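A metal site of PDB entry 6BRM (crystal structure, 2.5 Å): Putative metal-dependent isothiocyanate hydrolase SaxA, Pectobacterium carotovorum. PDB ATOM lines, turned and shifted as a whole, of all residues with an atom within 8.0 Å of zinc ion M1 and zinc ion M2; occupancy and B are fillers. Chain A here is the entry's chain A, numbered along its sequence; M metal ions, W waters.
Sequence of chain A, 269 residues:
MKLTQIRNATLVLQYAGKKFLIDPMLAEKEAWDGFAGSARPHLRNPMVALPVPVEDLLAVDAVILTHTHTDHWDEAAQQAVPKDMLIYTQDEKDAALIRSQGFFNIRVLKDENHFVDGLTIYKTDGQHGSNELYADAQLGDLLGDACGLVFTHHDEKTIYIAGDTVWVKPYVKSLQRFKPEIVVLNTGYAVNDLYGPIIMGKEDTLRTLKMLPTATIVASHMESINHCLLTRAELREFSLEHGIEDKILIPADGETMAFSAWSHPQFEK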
ATOM      1  N   ASN A   8     -23.434  23.209  39.821  1.00  0.00           N
ATOM      2  CA  ASN A   8     -23.354  23.087  38.362  1.00  0.00           C
ATOM      3  C   ASN A   8     -23.688  24.437  37.695  1.00  0.00           C
ATOM      4  O   ASN A   8     -22.899  25.363  37.828  1.00  0.00           O
ATOM      5  CB  ASN A   8     -24.166  21.891  37.848  1.00  0.00           C
ATOM      6  CG  ASN A   8     -23.872  21.568  36.388  1.00  0.00           C
ATOM      7  OD1 ASN A   8     -24.757  21.602  35.540  1.00  0.00           O
ATOM      8  ND2 ASN A   8     -22.621  21.255  36.089  1.00  0.00           N
ATOM      9  N   ALA A   9     -24.828  24.543  37.000  1.00  0.00           N
ATOM     10  CA  ALA A   9     -25.265  25.797  36.373  1.00  0.00           C
ATOM     11  C   ALA A   9     -26.500  26.392  37.071  1.00  0.00           C
ATOM     12  O   ALA A   9     -27.072  27.367  36.576  1.00  0.00           O
ATOM     13  CB  ALA A   9     -25.551  25.576  34.897  1.00  0.00           C
ATOM     14  N   ASP A  23     -31.930  27.372  35.815  1.00  0.00           N
ATOM     15  CA  ASP A  23     -31.572  25.958  35.621  1.00  0.00           C
ATOM     16  C   ASP A  23     -31.493  25.142  36.930  1.00  0.00           C
ATOM     17  O   ASP A  23     -30.424  24.662  37.300  1.00  0.00           O
ATOM     18  CB  ASP A  23     -30.249  25.866  34.839  1.00  0.00           C
ATOM     19  CG  ASP A  23     -30.312  26.561  33.481  1.00  0.00           C
ATOM     20  OD1 ASP A  23     -31.377  26.518  32.828  1.00  0.00           O
ATOM     21  OD2 ASP A  23     -29.300  27.158  33.056  1.00  0.00           O
ATOM     22  N   PHE A  35     -23.715  10.236  32.507  1.00  0.00           N
ATOM     23  CA  PHE A  35     -24.076  10.356  31.088  1.00  0.00           C
ATOM     24  C   PHE A  35     -23.382   9.295  30.223  1.00  0.00           C
ATOM     25  O   PHE A  35     -22.158   9.209  30.207  1.00  0.00           O
ATOM     26  CB  PHE A  35     -23.746  11.757  30.547  1.00  0.00           C
ATOM     27  CG  PHE A  35     -24.733  12.814  30.947  1.00  0.00           C
ATOM     28  CD1 PHE A  35     -25.932  12.955  30.252  1.00  0.00           C
ATOM     29  CD2 PHE A  35     -24.475  13.690  31.999  1.00  0.00           C
ATOM     30  CE1 PHE A  35     -26.849  13.937  30.598  1.00  0.00           C
ATOM     31  CE2 PHE A  35     -25.380  14.671  32.357  1.00  0.00           C
ATOM     32  CZ  PHE A  35     -26.575  14.789  31.656  1.00  0.00           C
ATOM     33  N   THR A  66     -32.851  27.482  30.555  1.00  0.00           N
ATOM     34  CA  THR A  66     -32.075  27.647  29.316  1.00  0.00           C
ATOM     35  C   THR A  66     -32.278  26.472  28.349  1.00  0.00           C
ATOM     36  O   THR A  66     -32.355  26.667  27.140  1.00  0.00           O
ATOM     37  CB  THR A  66     -30.572  27.832  29.586  1.00  0.00           C
ATOM     38  OG1 THR A  66     -30.069  26.707  30.327  1.00  0.00           O
ATOM     39  CG2 THR A  66     -30.314  29.113  30.374  1.00  0.00           C
ATOM     40  N   HIS A  67     -32.348  25.259  28.905  1.00  0.00           N
ATOM     41  CA  HIS A  67     -32.719  24.046  28.158  1.00  0.00           C
ATOM     42  C   HIS A  67     -33.069  22.910  29.130  1.00  0.00           C
ATOM     43  O   HIS A  67     -32.980  23.102  30.343  1.00  0.00           O
ATOM     44  CB  HIS A  67     -31.632  23.637  27.143  1.00  0.00           C
ATOM     45  CG  HIS A  67     -30.287  23.356  27.760  1.00  0.00           C
ATOM     46  ND1 HIS A  67     -29.642  24.244  28.592  1.00  0.00           N
ATOM     47  CD2 HIS A  67     -29.464  22.296  27.615  1.00  0.00           C
ATOM     48  CE1 HIS A  67     -28.478  23.727  28.954  1.00  0.00           C
ATOM     49  NE2 HIS A  67     -28.347  22.542  28.378  1.00  0.00           N
ATOM     50  N   THR A  68     -33.485  21.764  28.602  1.00  0.00           N
ATOM     51  CA  THR A  68     -34.021  20.664  29.412  1.00  0.00           C
ATOM     52  C   THR A  68     -33.105  19.422  29.489  1.00  0.00           C
ATOM     53  O   THR A  68     -33.598  18.291  29.534  1.00  0.00           O
ATOM     54  CB  THR A  68     -35.402  20.236  28.887  1.00  0.00           C
ATOM     55  OG1 THR A  68     -35.257  19.711  27.565  1.00  0.00           O
ATOM     56  CG2 THR A  68     -36.363  21.422  28.858  1.00  0.00           C
ATOM     57  N   HIS A  69     -31.788  19.636  29.508  1.00  0.00           N
ATOM     58  CA  HIS A  69     -30.839  18.568  29.892  1.00  0.00           C
ATOM     59  C   HIS A  69     -30.974  18.336  31.399  1.00  0.00           C
ATOM     60  O   HIS A  69     -31.359  19.244  32.139  1.00  0.00           O
ATOM     61  CB  HIS A  69     -29.390  18.919  29.529  1.00  0.00           C
ATOM     62  CG  HIS A  69     -29.086  18.783  28.057  1.00  0.00           C
ATOM     63  ND1 HIS A  69     -28.105  19.522  27.432  1.00  0.00           N
ATOM     64  CD2 HIS A  69     -29.614  17.981  27.105  1.00  0.00           C
ATOM     65  CE1 HIS A  69     -28.062  19.195  26.149  1.00  0.00           C
ATOM     66  NE2 HIS A  69     -28.968  18.258  25.929  1.00  0.00           N
ATOM     67  N   THR A  70     -30.646  17.127  31.838  1.00  0.00           N
ATOM     68  CA  THR A  70     -30.909  16.696  33.210  1.00  0.00           C
ATOM     69  C   THR A  70     -30.084  17.418  34.297  1.00  0.00           C
ATOM     70  O   THR A  70     -30.527  17.524  35.439  1.00  0.00           O
ATOM     71  CB  THR A  70     -30.716  15.176  33.358  1.00  0.00           C
ATOM     72  OG1 THR A  70     -31.306  14.513  32.225  1.00  0.00           O
ATOM     73  CG2 THR A  70     -31.372  14.646  34.630  1.00  0.00           C
ATOM     74  N   ASP A  71     -28.913  17.939  33.936  1.00  0.00           N
ATOM     75  CA  ASP A  71     -28.099  18.776  34.860  1.00  0.00           C
ATOM     76  C   ASP A  71     -28.612  20.224  35.008  1.00  0.00           C
ATOM     77  O   ASP A  71     -28.077  20.986  35.815  1.00  0.00           O
ATOM     78  CB  ASP A  71     -26.621  18.785  34.458  1.00  0.00           C
ATOM     79  CG  ASP A  71     -26.396  19.253  33.037  1.00  0.00           C
ATOM     80  OD1 ASP A  71     -27.039  18.669  32.141  1.00  0.00           O
ATOM     81  OD2 ASP A  71     -25.589  20.162  32.818  1.00  0.00           O
ATOM     82  N   HIS A  72     -29.614  20.605  34.203  1.00  0.00           N
ATOM     83  CA  HIS A  72     -30.300  21.892  34.306  1.00  0.00           C
ATOM     84  C   HIS A  72     -31.769  21.783  34.778  1.00  0.00           C
ATOM     85  O   HIS A  72     -32.361  22.781  35.163  1.00  0.00           O
ATOM     86  CB  HIS A  72     -30.251  22.599  32.944  1.00  0.00           C
ATOM     87  CG  HIS A  72     -28.853  22.853  32.462  1.00  0.00           C
ATOM     88  ND1 HIS A  72     -28.228  24.070  32.584  1.00  0.00           N
ATOM     89  CD2 HIS A  72     -27.956  22.031  31.853  1.00  0.00           C
ATOM     90  CE1 HIS A  72     -27.006  23.987  32.089  1.00  0.00           C
ATOM     91  NE2 HIS A  72     -26.816  22.759  31.637  1.00  0.00           N
ATOM     92  N   HIS A 128     -24.274  23.944  21.349  1.00  0.00           N
ATOM     93  CA  HIS A 128     -23.990  23.035  22.454  1.00  0.00           C
ATOM     94  C   HIS A 128     -23.263  21.799  21.906  1.00  0.00           C
ATOM     95  O   HIS A 128     -23.716  20.669  22.056  1.00  0.00           O
ATOM     96  CB  HIS A 128     -25.313  22.679  23.131  1.00  0.00           C
ATOM     97  CG  HIS A 128     -25.151  22.032  24.467  1.00  0.00           C
ATOM     98  ND1 HIS A 128     -23.970  21.455  24.892  1.00  0.00           N
ATOM     99  CD2 HIS A 128     -26.047  21.832  25.461  1.00  0.00           C
ATOM    100  CE1 HIS A 128     -24.144  20.949  26.099  1.00  0.00           C
ATOM    101  NE2 HIS A 128     -25.397  21.143  26.470  1.00  0.00           N
ATOM    102  N   LEU A 142     -30.266  15.481  20.299  1.00  0.00           N
ATOM    103  CA  LEU A 142     -29.932  15.181  21.697  1.00  0.00           C
ATOM    104  C   LEU A 142     -29.275  16.390  22.402  1.00  0.00           C
ATOM    105  O   LEU A 142     -29.670  16.752  23.513  1.00  0.00           O
ATOM    106  CB  LEU A 142     -29.048  13.935  21.802  1.00  0.00           C
ATOM    107  CG  LEU A 142     -29.267  13.040  23.035  1.00  0.00           C
ATOM    108  CD1 LEU A 142     -28.643  11.673  22.809  1.00  0.00           C
ATOM    109  CD2 LEU A 142     -28.754  13.685  24.318  1.00  0.00           C
ATOM    110  N   LEU A 143     -28.289  16.993  21.750  1.00  0.00           N
ATOM    111  CA  LEU A 143     -27.647  18.212  22.269  1.00  0.00           C
ATOM    112  C   LEU A 143     -28.566  19.435  22.115  1.00  0.00           C
ATOM    113  O   LEU A 143     -28.670  20.253  23.042  1.00  0.00           O
ATOM    114  CB  LEU A 143     -26.282  18.467  21.613  1.00  0.00           C
ATOM    115  CG  LEU A 143     -25.050  17.750  22.188  1.00  0.00           C
ATOM    116  CD1 LEU A 143     -24.801  18.136  23.642  1.00  0.00           C
ATOM    117  CD2 LEU A 143     -25.159  16.233  22.041  1.00  0.00           C
ATOM    118  N   GLY A 144     -29.200  19.553  20.953  1.00  0.00           N
ATOM    119  CA  GLY A 144     -30.291  20.503  20.733  1.00  0.00           C
ATOM    120  C   GLY A 144     -29.912  21.968  20.835  1.00  0.00           C
ATOM    121  O   GLY A 144     -28.771  22.338  20.540  1.00  0.00           O
ATOM    122  N   ASP A 145     -30.881  22.794  21.236  1.00  0.00           N
ATOM    123  CA  ASP A 145     -30.643  24.214  21.499  1.00  0.00           C
ATOM    124  C   ASP A 145     -30.420  24.422  22.994  1.00  0.00           C
ATOM    125  O   ASP A 145     -30.915  23.646  23.820  1.00  0.00           O
ATOM    126  CB  ASP A 145     -31.841  25.052  21.038  1.00  0.00           C
ATOM    127  CG  ASP A 145     -32.203  24.821  19.579  1.00  0.00           C
ATOM    128  OD1 ASP A 145     -31.393  24.216  18.834  1.00  0.00           O
ATOM    129  OD2 ASP A 145     -33.303  25.238  19.178  1.00  0.00           O
ATOM    130  N   ALA A 146     -29.698  25.486  23.342  1.00  0.00           N
ATOM    131  CA  ALA A 146     -29.492  25.879  24.731  1.00  0.00           C
ATOM    132  C   ALA A 146     -29.068  27.348  24.826  1.00  0.00           C
ATOM    133  O   ALA A 146     -27.909  27.675  24.560  1.00  0.00           O
ATOM    134  CB  ALA A 146     -28.458  24.978  25.397  1.00  0.00           C
ATOM    135  N   GLY A 163     -24.637  30.276  28.958  1.00  0.00           N
ATOM    136  CA  GLY A 163     -25.278  28.953  28.793  1.00  0.00           C
ATOM    137  C   GLY A 163     -24.370  27.878  28.219  1.00  0.00           C
ATOM    138  O   GLY A 163     -23.193  28.121  27.959  1.00  0.00           O
ATOM    139  N   ASP A 164     -24.926  26.678  28.027  1.00  0.00           N
ATOM    140  CA  ASP A 164     -24.192  25.557  27.429  1.00  0.00           C
ATOM    141  C   ASP A 164     -23.920  25.800  25.949  1.00  0.00           C
ATOM    142  O   ASP A 164     -24.677  25.377  25.078  1.00  0.00           O
ATOM    143  CB  ASP A 164     -24.979  24.243  27.579  1.00  0.00           C
ATOM    144  CG  ASP A 164     -24.982  23.690  28.999  1.00  0.00           C
ATOM    145  OD1 ASP A 164     -24.643  24.415  29.952  1.00  0.00           O
ATOM    146  OD2 ASP A 164     -25.338  22.502  29.145  1.00  0.00           O
ATOM    147  N   THR A 165     -22.804  26.487  25.678  1.00  0.00           N
ATOM    148  CA  THR A 165     -22.354  26.777  24.324  1.00  0.00           C
ATOM    149  C   THR A 165     -20.830  26.702  24.235  1.00  0.00           C
ATOM    150  O   THR A 165     -20.159  27.009  25.222  1.00  0.00           O
ATOM    151  CB  THR A 165     -22.838  28.171  23.862  1.00  0.00           C
ATOM    152  OG1 THR A 165     -22.498  28.372  22.486  1.00  0.00           O
ATOM    153  CG2 THR A 165     -22.240  29.299  24.710  1.00  0.00           C
ATOM    154  N   ASN A 186     -20.265  28.743  31.259  1.00  0.00           N
ATOM    155  CA  ASN A 186     -20.305  27.344  31.656  1.00  0.00           C
ATOM    156  C   ASN A 186     -18.998  26.691  31.197  1.00  0.00           C
ATOM    157  O   ASN A 186     -18.900  26.181  30.082  1.00  0.00           O
ATOM    158  CB  ASN A 186     -21.543  26.651  31.055  1.00  0.00           C
ATOM    159  CG  ASN A 186     -22.836  27.232  31.589  1.00  0.00           C
ATOM    160  OD1 ASN A 186     -22.842  28.217  32.321  1.00  0.00           O
ATOM    161  ND2 ASN A 186     -23.950  26.623  31.216  1.00  0.00           N
ATOM    162  N   ALA A 190     -16.936  19.724  29.277  1.00  0.00           N
ATOM    163  CA  ALA A 190     -17.602  18.426  29.187  1.00  0.00           C
ATOM    164  C   ALA A 190     -17.250  17.748  27.875  1.00  0.00           C
ATOM    165  O   ALA A 190     -17.454  18.315  26.805  1.00  0.00           O
ATOM    166  CB  ALA A 190     -19.101  18.577  29.325  1.00  0.00           C
ATOM    167  N   ILE A 198     -18.286  19.696  24.399  1.00  0.00           N
ATOM    168  CA  ILE A 198     -19.657  20.174  24.142  1.00  0.00           C
ATOM    169  C   ILE A 198     -19.971  21.550  24.754  1.00  0.00           C
ATOM    170  O   ILE A 198     -20.953  22.172  24.375  1.00  0.00           O
ATOM    171  CB  ILE A 198     -20.753  19.153  24.555  1.00  0.00           C
ATOM    172  CG1 ILE A 198     -20.789  18.917  26.080  1.00  0.00           C
ATOM    173  CG2 ILE A 198     -20.545  17.839  23.824  1.00  0.00           C
ATOM    174  CD1 ILE A 198     -21.957  18.067  26.540  1.00  0.00           C
ATOM    175  N   ILE A 199     -19.143  21.999  25.696  1.00  0.00           N
ATOM    176  CA  ILE A 199     -19.223  23.345  26.298  1.00  0.00           C
ATOM    177  C   ILE A 199     -17.809  23.918  26.494  1.00  0.00           C
ATOM    178  O   ILE A 199     -16.818  23.250  26.189  1.00  0.00           O
ATOM    179  CB  ILE A 199     -20.032  23.347  27.617  1.00  0.00           C
ATOM    180  CG1 ILE A 199     -19.378  22.454  28.684  1.00  0.00           C
ATOM    181  CG2 ILE A 199     -21.471  22.882  27.380  1.00  0.00           C
ATOM    182  CD1 ILE A 199     -20.001  22.579  30.065  1.00  0.00           C
ATOM    183  N   HIS A 221     -20.689  25.725  36.068  1.00  0.00           N
ATOM    184  CA  HIS A 221     -20.886  24.416  35.411  1.00  0.00           C
ATOM    185  C   HIS A 221     -19.685  23.481  35.646  1.00  0.00           C
ATOM    186  O   HIS A 221     -19.293  22.737  34.745  1.00  0.00           O
ATOM    187  CB  HIS A 221     -21.204  24.592  33.904  1.00  0.00           C
ATOM    188  CG  HIS A 221     -22.047  23.494  33.319  1.00  0.00           C
ATOM    189  ND1 HIS A 221     -21.660  22.178  33.313  1.00  0.00           N
ATOM    190  CD2 HIS A 221     -23.242  23.541  32.682  1.00  0.00           C
ATOM    191  CE1 HIS A 221     -22.592  21.456  32.717  1.00  0.00           C
ATOM    192  NE2 HIS A 221     -23.563  22.261  32.307  1.00  0.00           N
ATOM    193  N   ILE A 225     -21.115  17.429  37.434  1.00  0.00           N
ATOM    194  CA  ILE A 225     -21.485  16.400  36.462  1.00  0.00           C
ATOM    195  C   ILE A 225     -20.246  15.618  36.061  1.00  0.00           C
ATOM    196  O   ILE A 225     -19.137  16.168  36.017  1.00  0.00           O
ATOM    197  CB  ILE A 225     -22.164  17.043  35.224  1.00  0.00           C
ATOM    198  CG1 ILE A 225     -23.330  17.954  35.658  1.00  0.00           C
ATOM    199  CG2 ILE A 225     -22.670  15.986  34.258  1.00  0.00           C
ATOM    200  CD1 ILE A 225     -24.385  17.292  36.529  1.00  0.00           C
ATOM    201  N   HIS A 227     -18.956  14.211  33.281  1.00  0.00           N
ATOM    202  CA  HIS A 227     -18.144  14.471  32.088  1.00  0.00           C
ATOM    203  C   HIS A 227     -17.389  15.810  32.095  1.00  0.00           C
ATOM    204  O   HIS A 227     -16.534  16.028  31.248  1.00  0.00           O
ATOM    205  CB  HIS A 227     -18.926  14.274  30.769  1.00  0.00           C
ATOM    206  CG  HIS A 227     -20.178  15.092  30.653  1.00  0.00           C
ATOM    207  ND1 HIS A 227     -20.333  16.317  31.261  1.00  0.00           N
ATOM    208  CD2 HIS A 227     -21.309  14.873  29.945  1.00  0.00           C
ATOM    209  CE1 HIS A 227     -21.523  16.805  30.953  1.00  0.00           C
ATOM    210  NE2 HIS A 227     -22.129  15.950  30.158  1.00  0.00           N
ATOM    211  N   CYS A 228     -17.695  16.685  33.060  1.00  0.00           N
ATOM    212  CA  CYS A 228     -16.975  17.959  33.209  1.00  0.00           C
ATOM    213  C   CYS A 228     -15.605  17.752  33.865  1.00  0.00           C
ATOM    214  O   CYS A 228     -15.511  17.569  35.074  1.00  0.00           O
ATOM    215  CB  CYS A 228     -17.815  18.947  34.016  1.00  0.00           C
ATOM    216  SG  CYS A 228     -19.297  19.495  33.139  1.00  0.00           S
HETATM  217 ZN    ZN M   1     -25.177  21.419  31.046  1.00  0.00          ZN
HETATM  218 ZN    ZN M   2     -26.726  21.043  28.221  1.00  0.00          ZN
HETATM  219  O   HOH W   1     -26.336  19.856  30.014  1.00  0.00           O
HETATM  220  O   HOH W   2     -23.669  19.993  30.289  1.00  0.00           O
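N of His 221 is in hydrogen-bond range of O of Asn 8.
The side-chain carboxylate (OD2) of Asp 23 sits at hydrogen-bond distance from a ring nitrogen (ND1) of His 72, at 3.3 Å.
The side-chain carboxylate (OD1) of Asp 164 lies within hydrogen-bond range of the side-chain amide nitrogen (ND2) of Asn 186, at 2.6 Å.
A ring nitrogen (NE2) of His 69 lies within hydrogen-bond range of the backbone carbonyl oxygen (O) of Leu 142 (2.9 Å).
O of Asp 71 lies close to OD1 of Asn 8 (3.4 Å).
The side-chain sulfur (SG) of Cys 228 lies within hydrogen-bond range of a ring nitrogen (ND1) of His 221, at 3.6 Å.
A ring nitrogen (ND1) of His 67 sits at hydrogen-bond distance from the side-chain hydroxyl (OG1) of Thr 66 (3.0 Å).
The backbone carbonyl oxygen (O) of Ile 198 sits at hydrogen-bond distance from a ring nitrogen (ND1) of His 128 (3.1 Å).
Along chain A the residues within 4 Å of zinc ion M1 span positions 71 to 221.
The nearest printed residue that does not touch zinc ion M1 is His 67 (4.3 Å).
Of the 28 residues printed, 5 come within 4 Å of zinc ion M2.
Zinc ion M1 is bound by the side-chain carboxylate (OD2) of Asp 164 (2.2 Å), a ring nitrogen (NE2) of His 72 (2.2 Å), water W1 (2.2 Å), water W2 (2.2 Å), the side-chain carboxylate (OD2) of Asp 71 (2.2 Å) and a ring nitrogen (NE2) of His 221 (2.2 Å).
Zinc ion M1 has six donor atoms within binding distance.
Zinc ion M2 is bound by water W1 (2.2 Å), ND1 of His 69 (2.2 Å), NE2 of His 128 (2.2 Å), NE2 of His 67 (2.2 Å) and OD2 of Asp 164 (2.2 Å).
Zinc ion M2 has five donor atoms within binding distance.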
